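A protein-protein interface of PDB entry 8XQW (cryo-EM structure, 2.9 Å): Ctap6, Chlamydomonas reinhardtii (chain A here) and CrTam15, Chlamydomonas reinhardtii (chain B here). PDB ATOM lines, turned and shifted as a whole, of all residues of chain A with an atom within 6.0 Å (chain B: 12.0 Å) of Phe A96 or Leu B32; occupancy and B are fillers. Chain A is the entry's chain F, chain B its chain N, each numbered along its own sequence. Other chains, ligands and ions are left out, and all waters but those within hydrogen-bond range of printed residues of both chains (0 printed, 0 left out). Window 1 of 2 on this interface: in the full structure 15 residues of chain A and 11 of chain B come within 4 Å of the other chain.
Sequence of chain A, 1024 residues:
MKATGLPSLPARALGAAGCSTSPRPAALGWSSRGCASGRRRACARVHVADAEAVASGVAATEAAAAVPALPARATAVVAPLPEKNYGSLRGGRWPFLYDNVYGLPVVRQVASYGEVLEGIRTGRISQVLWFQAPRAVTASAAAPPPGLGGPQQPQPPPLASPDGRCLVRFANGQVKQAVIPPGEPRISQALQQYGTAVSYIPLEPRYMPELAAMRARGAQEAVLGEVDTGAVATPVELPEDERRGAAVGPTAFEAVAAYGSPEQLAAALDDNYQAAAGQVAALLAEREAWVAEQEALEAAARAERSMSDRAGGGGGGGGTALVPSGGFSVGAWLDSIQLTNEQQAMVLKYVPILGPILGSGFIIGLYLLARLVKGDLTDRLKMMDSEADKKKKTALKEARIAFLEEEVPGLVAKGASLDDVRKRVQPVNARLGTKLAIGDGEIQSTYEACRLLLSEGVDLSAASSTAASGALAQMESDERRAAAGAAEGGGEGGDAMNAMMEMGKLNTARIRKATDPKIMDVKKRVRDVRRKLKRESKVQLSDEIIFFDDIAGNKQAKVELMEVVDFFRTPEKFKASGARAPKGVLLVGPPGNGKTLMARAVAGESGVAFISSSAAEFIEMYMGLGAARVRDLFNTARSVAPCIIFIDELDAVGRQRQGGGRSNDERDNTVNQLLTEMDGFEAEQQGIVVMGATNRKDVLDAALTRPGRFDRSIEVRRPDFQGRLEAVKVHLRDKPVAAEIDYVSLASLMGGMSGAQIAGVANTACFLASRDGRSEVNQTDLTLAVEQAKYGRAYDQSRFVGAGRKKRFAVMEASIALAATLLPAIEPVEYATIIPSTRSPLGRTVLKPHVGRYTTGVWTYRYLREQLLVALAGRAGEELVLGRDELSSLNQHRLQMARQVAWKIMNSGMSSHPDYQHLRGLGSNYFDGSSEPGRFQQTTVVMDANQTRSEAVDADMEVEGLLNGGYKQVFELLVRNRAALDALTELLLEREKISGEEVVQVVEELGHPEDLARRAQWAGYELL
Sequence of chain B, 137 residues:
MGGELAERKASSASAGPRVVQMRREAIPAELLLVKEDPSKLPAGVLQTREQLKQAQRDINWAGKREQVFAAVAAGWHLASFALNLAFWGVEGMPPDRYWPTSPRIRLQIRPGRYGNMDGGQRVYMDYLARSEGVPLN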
ATOM      1  N   ALA A  74     -10.243   5.863 -13.845  1.00  0.00           N
ATOM      2  CA  ALA A  74     -10.812   7.096 -14.366  1.00  0.00           C
ATOM      3  C   ALA A  74      -9.710   8.140 -14.515  1.00  0.00           C
ATOM      4  O   ALA A  74      -8.627   8.024 -13.941  1.00  0.00           O
ATOM      5  CB  ALA A  74     -11.938   7.605 -13.462  1.00  0.00           C
ATOM      6  N   VAL A  78      -8.060  17.999 -12.497  1.00  0.00           N
ATOM      7  CA  VAL A  78      -8.357  18.327 -11.110  1.00  0.00           C
ATOM      8  C   VAL A  78      -7.645  19.623 -10.755  1.00  0.00           C
ATOM      9  O   VAL A  78      -6.628  19.978 -11.358  1.00  0.00           O
ATOM     10  CB  VAL A  78      -7.928  17.188 -10.160  1.00  0.00           C
ATOM     11  CG1 VAL A  78      -8.737  17.228  -8.877  1.00  0.00           C
ATOM     12  CG2 VAL A  78      -8.065  15.845 -10.847  1.00  0.00           C
ATOM     13  N   ARG A  93      -2.157  20.370  -0.401  1.00  0.00           N
ATOM     14  CA  ARG A  93      -2.605  20.633  -1.758  1.00  0.00           C
ATOM     15  C   ARG A  93      -3.086  19.383  -2.470  1.00  0.00           C
ATOM     16  O   ARG A  93      -3.602  19.485  -3.584  1.00  0.00           O
ATOM     17  CB  ARG A  93      -1.483  21.270  -2.569  1.00  0.00           C
ATOM     18  CG  ARG A  93      -0.774  22.376  -1.846  1.00  0.00           C
ATOM     19  CD  ARG A  93       0.399  22.856  -2.655  1.00  0.00           C
ATOM     20  NE  ARG A  93      -0.014  23.783  -3.698  1.00  0.00           N
ATOM     21  CZ  ARG A  93       0.622  23.928  -4.852  1.00  0.00           C
ATOM     22  NH1 ARG A  93       0.181  24.798  -5.749  1.00  0.00           N
ATOM     23  NH2 ARG A  93       1.697  23.197  -5.110  1.00  0.00           N
ATOM     24  N   TRP A  94      -2.916  18.220  -1.873  1.00  0.00           N
ATOM     25  CA  TRP A  94      -3.463  16.998  -2.438  1.00  0.00           C
ATOM     26  C   TRP A  94      -4.981  17.085  -2.434  1.00  0.00           C
ATOM     27  O   TRP A  94      -5.580  17.176  -1.357  1.00  0.00           O
ATOM     28  CB  TRP A  94      -3.001  15.803  -1.627  1.00  0.00           C
ATOM     29  CG  TRP A  94      -3.093  14.509  -2.336  1.00  0.00           C
ATOM     30  CD1 TRP A  94      -3.818  13.425  -1.959  1.00  0.00           C
ATOM     31  CD2 TRP A  94      -2.422  14.145  -3.540  1.00  0.00           C
ATOM     32  NE1 TRP A  94      -3.645  12.404  -2.857  1.00  0.00           N
ATOM     33  CE2 TRP A  94      -2.789  12.822  -3.837  1.00  0.00           C
ATOM     34  CE3 TRP A  94      -1.545  14.808  -4.393  1.00  0.00           C
ATOM     35  CZ2 TRP A  94      -2.318  12.154  -4.953  1.00  0.00           C
ATOM     36  CZ3 TRP A  94      -1.081  14.145  -5.500  1.00  0.00           C
ATOM     37  CH2 TRP A  94      -1.466  12.832  -5.774  1.00  0.00           C
ATOM     38  N   PRO A  95      -5.641  17.073  -3.591  1.00  0.00           N
ATOM     39  CA  PRO A  95      -7.101  17.192  -3.626  1.00  0.00           C
ATOM     40  C   PRO A  95      -7.851  15.878  -3.501  1.00  0.00           C
ATOM     41  O   PRO A  95      -9.079  15.902  -3.367  1.00  0.00           O
ATOM     42  CB  PRO A  95      -7.330  17.807  -5.005  1.00  0.00           C
ATOM     43  CG  PRO A  95      -6.281  17.192  -5.832  1.00  0.00           C
ATOM     44  CD  PRO A  95      -5.074  17.021  -4.948  1.00  0.00           C
ATOM     45  N   PHE A  96      -7.166  14.745  -3.535  1.00  0.00           N
ATOM     46  CA  PHE A  96      -7.809  13.447  -3.464  1.00  0.00           C
ATOM     47  C   PHE A  96      -7.948  13.006  -2.016  1.00  0.00           C
ATOM     48  O   PHE A  96      -7.438  13.643  -1.094  1.00  0.00           O
ATOM     49  CB  PHE A  96      -7.015  12.402  -4.242  1.00  0.00           C
ATOM     50  CG  PHE A  96      -6.796  12.760  -5.672  1.00  0.00           C
ATOM     51  CD1 PHE A  96      -7.842  12.750  -6.566  1.00  0.00           C
ATOM     52  CD2 PHE A  96      -5.542  13.107  -6.125  1.00  0.00           C
ATOM     53  CE1 PHE A  96      -7.638  13.072  -7.887  1.00  0.00           C
ATOM     54  CE2 PHE A  96      -5.334  13.434  -7.443  1.00  0.00           C
ATOM     55  CZ  PHE A  96      -6.382  13.416  -8.325  1.00  0.00           C
ATOM     56  N   LEU A  97      -8.660  11.904  -1.826  1.00  0.00           N
ATOM     57  CA  LEU A  97      -8.772  11.308  -0.507  1.00  0.00           C
ATOM     58  C   LEU A  97      -7.868  10.104  -0.330  1.00  0.00           C
ATOM     59  O   LEU A  97      -7.792   9.564   0.776  1.00  0.00           O
ATOM     60  CB  LEU A  97     -10.219  10.899  -0.231  1.00  0.00           C
ATOM     61  CG  LEU A  97     -11.123  11.997   0.323  1.00  0.00           C
ATOM     62  CD1 LEU A  97     -12.550  11.510   0.400  1.00  0.00           C
ATOM     63  CD2 LEU A  97     -10.646  12.460   1.685  1.00  0.00           C
ATOM     64  N   TYR A  98      -7.201   9.664  -1.390  1.00  0.00           N
ATOM     65  CA  TYR A  98      -6.330   8.500  -1.364  1.00  0.00           C
ATOM     66  C   TYR A  98      -5.014   8.842  -2.049  1.00  0.00           C
ATOM     67  O   TYR A  98      -4.882   9.878  -2.703  1.00  0.00           O
ATOM     68  CB  TYR A  98      -7.000   7.297  -2.040  1.00  0.00           C
ATOM     69  CG  TYR A  98      -8.353   6.949  -1.461  1.00  0.00           C
ATOM     70  CD1 TYR A  98      -9.463   7.738  -1.715  1.00  0.00           C
ATOM     71  CD2 TYR A  98      -8.518   5.833  -0.664  1.00  0.00           C
ATOM     72  CE1 TYR A  98     -10.687   7.432  -1.186  1.00  0.00           C
ATOM     73  CE2 TYR A  98      -9.746   5.516  -0.134  1.00  0.00           C
ATOM     74  CZ  TYR A  98     -10.826   6.319  -0.397  1.00  0.00           C
ATOM     75  OH  TYR A  98     -12.054   6.008   0.131  1.00  0.00           O
ATOM     76  N   ASP A  99      -4.033   7.966  -1.896  1.00  0.00           N
ATOM     77  CA  ASP A  99      -2.687   8.242  -2.374  1.00  0.00           C
ATOM     78  C   ASP A  99      -2.359   7.381  -3.589  1.00  0.00           C
ATOM     79  O   ASP A  99      -3.155   6.559  -4.042  1.00  0.00           O
ATOM     80  CB  ASP A  99      -1.667   8.033  -1.255  1.00  0.00           C
ATOM     81  CG  ASP A  99      -1.229   6.598  -1.128  1.00  0.00           C
ATOM     82  OD1 ASP A  99      -0.321   6.174  -1.876  1.00  0.00           O
ATOM     83  OD2 ASP A  99      -1.792   5.889  -0.271  1.00  0.00           O
ATOM     84  N   ASN A 100      -1.152   7.577  -4.114  1.00  0.00           N
ATOM     85  CA  ASN A 100      -0.771   6.959  -5.377  1.00  0.00           C
ATOM     86  C   ASN A 100      -0.309   5.519  -5.189  1.00  0.00           C
ATOM     87  O   ASN A 100      -0.893   4.592  -5.756  1.00  0.00           O
ATOM     88  CB  ASN A 100       0.328   7.784  -6.040  1.00  0.00           C
ATOM     89  CG  ASN A 100      -0.052   9.226  -6.188  1.00  0.00           C
ATOM     90  OD1 ASN A 100      -1.120   9.545  -6.704  1.00  0.00           O
ATOM     91  ND2 ASN A 100       0.812  10.117  -5.723  1.00  0.00           N
ATOM     92  N   VAL A 106      -5.775   9.427   3.284  1.00  0.00           N
ATOM     93  CA  VAL A 106      -4.739  10.321   3.777  1.00  0.00           C
ATOM     94  C   VAL A 106      -5.287  11.121   4.946  1.00  0.00           C
ATOM     95  O   VAL A 106      -6.382  11.687   4.870  1.00  0.00           O
ATOM     96  CB  VAL A 106      -4.249  11.244   2.649  1.00  0.00           C
ATOM     97  CG1 VAL A 106      -3.410  12.364   3.204  1.00  0.00           C
ATOM     98  CG2 VAL A 106      -3.476  10.455   1.624  1.00  0.00           C
ATOM     99  N   ARG A 108      -5.466  14.391   7.034  1.00  0.00           N
ATOM    100  CA  ARG A 108      -5.282  15.775   6.633  1.00  0.00           C
ATOM    101  C   ARG A 108      -5.735  16.778   7.680  1.00  0.00           C
ATOM    102  O   ARG A 108      -5.882  17.961   7.358  1.00  0.00           O
ATOM    103  CB  ARG A 108      -6.006  16.037   5.312  1.00  0.00           C
ATOM    104  CG  ARG A 108      -7.440  15.557   5.279  1.00  0.00           C
ATOM    105  CD  ARG A 108      -8.194  16.133   4.088  1.00  0.00           C
ATOM    106  NE  ARG A 108      -7.800  17.505   3.795  1.00  0.00           N
ATOM    107  CZ  ARG A 108      -7.001  17.857   2.794  1.00  0.00           C
ATOM    108  NH1 ARG A 108      -6.499  16.933   1.989  1.00  0.00           N
ATOM    109  NH2 ARG A 108      -6.693  19.132   2.604  1.00  0.00           N
ATOM    110  N   GLU B  25     -14.688  -1.824 -13.112  1.00  0.00           N
ATOM    111  CA  GLU B  25     -15.700  -1.270 -12.230  1.00  0.00           C
ATOM    112  C   GLU B  25     -15.544   0.244 -12.216  1.00  0.00           C
ATOM    113  O   GLU B  25     -14.528   0.788 -12.656  1.00  0.00           O
ATOM    114  CB  GLU B  25     -15.589  -1.847 -10.813  1.00  0.00           C
ATOM    115  CG  GLU B  25     -14.167  -1.910 -10.283  1.00  0.00           C
ATOM    116  CD  GLU B  25     -14.006  -2.894  -9.140  1.00  0.00           C
ATOM    117  OE1 GLU B  25     -13.282  -3.897  -9.314  1.00  0.00           O
ATOM    118  OE2 GLU B  25     -14.596  -2.663  -8.066  1.00  0.00           O
ATOM    119  N   ALA B  26     -16.563   0.932 -11.714  1.00  0.00           N
ATOM    120  CA  ALA B  26     -16.587   2.384 -11.751  1.00  0.00           C
ATOM    121  C   ALA B  26     -16.733   2.944 -10.346  1.00  0.00           C
ATOM    122  O   ALA B  26     -17.432   2.379  -9.502  1.00  0.00           O
ATOM    123  CB  ALA B  26     -17.725   2.903 -12.639  1.00  0.00           C
ATOM    124  N   ILE B  27     -16.065   4.068 -10.109  1.00  0.00           N
ATOM    125  CA  ILE B  27     -16.103   4.735  -8.812  1.00  0.00           C
ATOM    126  C   ILE B  27     -16.599   6.164  -9.002  1.00  0.00           C
ATOM    127  O   ILE B  27     -16.062   6.901  -9.842  1.00  0.00           O
ATOM    128  CB  ILE B  27     -14.725   4.710  -8.133  1.00  0.00           C
ATOM    129  CG1 ILE B  27     -14.311   3.270  -7.826  1.00  0.00           C
ATOM    130  CG2 ILE B  27     -14.737   5.559  -6.872  1.00  0.00           C
ATOM    131  CD1 ILE B  27     -14.686   2.803  -6.442  1.00  0.00           C
ATOM    132  N   PRO B  28     -17.613   6.592  -8.254  1.00  0.00           N
ATOM    133  CA  PRO B  28     -18.112   7.965  -8.398  1.00  0.00           C
ATOM    134  C   PRO B  28     -17.035   8.987  -8.067  1.00  0.00           C
ATOM    135  O   PRO B  28     -16.388   8.920  -7.022  1.00  0.00           O
ATOM    136  CB  PRO B  28     -19.270   8.027  -7.397  1.00  0.00           C
ATOM    137  CG  PRO B  28     -19.684   6.613  -7.209  1.00  0.00           C
ATOM    138  CD  PRO B  28     -18.426   5.807  -7.314  1.00  0.00           C
ATOM    139  N   ALA B  29     -16.862   9.948  -8.966  1.00  0.00           N
ATOM    140  CA  ALA B  29     -15.821  10.958  -8.810  1.00  0.00           C
ATOM    141  C   ALA B  29     -16.100  11.922  -7.697  1.00  0.00           C
ATOM    142  O   ALA B  29     -15.297  12.833  -7.491  1.00  0.00           O
ATOM    143  CB  ALA B  29     -15.629  11.719 -10.122  1.00  0.00           C
ATOM    144  N   GLU B  30     -17.206  11.784  -6.974  1.00  0.00           N
ATOM    145  CA  GLU B  30     -17.416  12.530  -5.744  1.00  0.00           C
ATOM    146  C   GLU B  30     -17.018  11.728  -4.519  1.00  0.00           C
ATOM    147  O   GLU B  30     -16.999  12.271  -3.413  1.00  0.00           O
ATOM    148  CB  GLU B  30     -18.878  12.971  -5.627  1.00  0.00           C
ATOM    149  CG  GLU B  30     -19.865  11.840  -5.400  1.00  0.00           C
ATOM    150  CD  GLU B  30     -20.390  11.807  -3.979  1.00  0.00           C
ATOM    151  OE1 GLU B  30     -21.417  11.144  -3.740  1.00  0.00           O
ATOM    152  OE2 GLU B  30     -19.772  12.444  -3.102  1.00  0.00           O
ATOM    153  N   LEU B  31     -16.701  10.448  -4.696  1.00  0.00           N
ATOM    154  CA  LEU B  31     -16.112   9.630  -3.650  1.00  0.00           C
ATOM    155  C   LEU B  31     -14.590   9.621  -3.716  1.00  0.00           C
ATOM    156  O   LEU B  31     -13.956   8.790  -3.061  1.00  0.00           O
ATOM    157  CB  LEU B  31     -16.649   8.200  -3.735  1.00  0.00           C
ATOM    158  CG  LEU B  31     -18.113   7.973  -3.354  1.00  0.00           C
ATOM    159  CD1 LEU B  31     -18.486   6.513  -3.531  1.00  0.00           C
ATOM    160  CD2 LEU B  31     -18.380   8.418  -1.930  1.00  0.00           C
ATOM    161  N   LEU B  32     -13.992  10.525  -4.494  1.00  0.00           N
ATOM    162  CA  LEU B  32     -12.547  10.597  -4.639  1.00  0.00           C
ATOM    163  C   LEU B  32     -11.961  11.975  -4.393  1.00  0.00           C
ATOM    164  O   LEU B  32     -10.735  12.111  -4.421  1.00  0.00           O
ATOM    165  CB  LEU B  32     -12.120  10.144  -6.043  1.00  0.00           C
ATOM    166  CG  LEU B  32     -12.238   8.666  -6.401  1.00  0.00           C
ATOM    167  CD1 LEU B  32     -11.389   8.368  -7.622  1.00  0.00           C
ATOM    168  CD2 LEU B  32     -11.831   7.782  -5.243  1.00  0.00           C
ATOM    169  N   LEU B  33     -12.777  12.997  -4.180  1.00  0.00           N
ATOM    170  CA  LEU B  33     -12.280  14.353  -3.999  1.00  0.00           C
ATOM    171  C   LEU B  33     -12.790  14.936  -2.690  1.00  0.00           C
ATOM    172  O   LEU B  33     -13.931  14.688  -2.290  1.00  0.00           O
ATOM    173  CB  LEU B  33     -12.700  15.247  -5.165  1.00  0.00           C
ATOM    174  CG  LEU B  33     -12.225  14.812  -6.551  1.00  0.00           C
ATOM    175  CD1 LEU B  33     -12.747  15.754  -7.619  1.00  0.00           C
ATOM    176  CD2 LEU B  33     -10.717  14.746  -6.595  1.00  0.00           C
ATOM    177  N   VAL B  34     -11.943  15.712  -2.030  1.00  0.00           N
ATOM    178  CA  VAL B  34     -12.331  16.352  -0.781  1.00  0.00           C
ATOM    179  C   VAL B  34     -13.164  17.586  -1.089  1.00  0.00           C
ATOM    180  O   VAL B  34     -13.103  18.152  -2.186  1.00  0.00           O
ATOM    181  CB  VAL B  34     -11.095  16.694   0.074  1.00  0.00           C
ATOM    182  CG1 VAL B  34      -9.925  15.809  -0.311  1.00  0.00           C
ATOM    183  CG2 VAL B  34     -10.726  18.166  -0.064  1.00  0.00           C
ATOM    184  N   LYS B  35     -13.961  17.998  -0.113  1.00  0.00           N
ATOM    185  CA  LYS B  35     -14.931  19.074  -0.276  1.00  0.00           C
ATOM    186  C   LYS B  35     -14.891  19.965   0.956  1.00  0.00           C
ATOM    187  O   LYS B  35     -15.477  19.625   1.989  1.00  0.00           O
ATOM    188  CB  LYS B  35     -16.330  18.505  -0.486  1.00  0.00           C
ATOM    189  CG  LYS B  35     -16.549  17.175   0.223  1.00  0.00           C
ATOM    190  CD  LYS B  35     -17.562  16.315  -0.512  1.00  0.00           C
ATOM    191  CE  LYS B  35     -17.206  16.176  -1.979  1.00  0.00           C
ATOM    192  NZ  LYS B  35     -18.169  15.296  -2.693  1.00  0.00           N
ATOM    193  N   GLU B  36     -14.199  21.093   0.855  1.00  0.00           N
ATOM    194  CA  GLU B  36     -14.237  22.105   1.894  1.00  0.00           C
ATOM    195  C   GLU B  36     -13.821  23.443   1.304  1.00  0.00           C
ATOM    196  O   GLU B  36     -12.960  23.513   0.425  1.00  0.00           O
ATOM    197  CB  GLU B  36     -13.336  21.734   3.074  1.00  0.00           C
ATOM    198  CG  GLU B  36     -13.631  22.520   4.341  1.00  0.00           C
ATOM    199  CD  GLU B  36     -12.677  23.675   4.562  1.00  0.00           C
ATOM    200  OE1 GLU B  36     -12.150  24.224   3.572  1.00  0.00           O
ATOM    201  OE2 GLU B  36     -12.451  24.034   5.735  1.00  0.00           O
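Among the printed residues, pairs that only touch across the chains: Val A78 with Leu B33 (3.9 Å), Pro A95 with Leu B33 (3.6 Å), Phe A96 with Leu B32 (3.4 Å), Phe A96 with Leu B33 (3.5 Å), Phe A96 with Val B34 (3.4 Å) and Leu A97 with Val B34 (3.96 Å).
The backbone NH (N) of Val A106 sits at hydrogen-bond distance from the backbone carbonyl oxygen (O) of Leu A97 (3.2 Å).
The backbone NH of Val B34 lies within hydrogen-bond range of the backbone carbonyl oxygen of Pro A95 (3.2 Å).
The backbone carbonyl oxygen (O) of Leu B32 is in hydrogen-bond range of the backbone NH (N) of Leu A97 (3.3 Å).
Of the 12 printed residues of chain B, 3 touch a printed residue of chain A.
Hydrophobic or aromatic side chains of chain A that line the printed part of chain B: Val A78, Phe A96 and Leu A97.
Among the printed residues, 8 pairs touch across the chains.
Among the printed residues, no Asp or Glu carboxylate lies within 4 Å of a Lys or Arg side-chain nitrogen of the other chain.
Val A78 touches just one residue of chain B: Leu B33 (3.9 Å).
Arg A93 touches none of the printed residues of chain B.
Phe A96 touches just these residues of chain B: Leu B32 (3.4 Å), Leu B33 (3.5 Å) and Val B34 (3.4 Å).
Val A106 touches none of the printed residues of chain B.
Of the printed residues of chain A, Leu B33 touches Val A78, Pro A95 and Phe A96.
Of the printed residues of chain A, Val B34 touches Pro A95 (3.2 Å), Phe A96 (3.4 Å) and Leu A97 (3.96 Å).
The nearest residue of chain B that does not touch Phe A96 is Leu B31 (7.4 Å).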
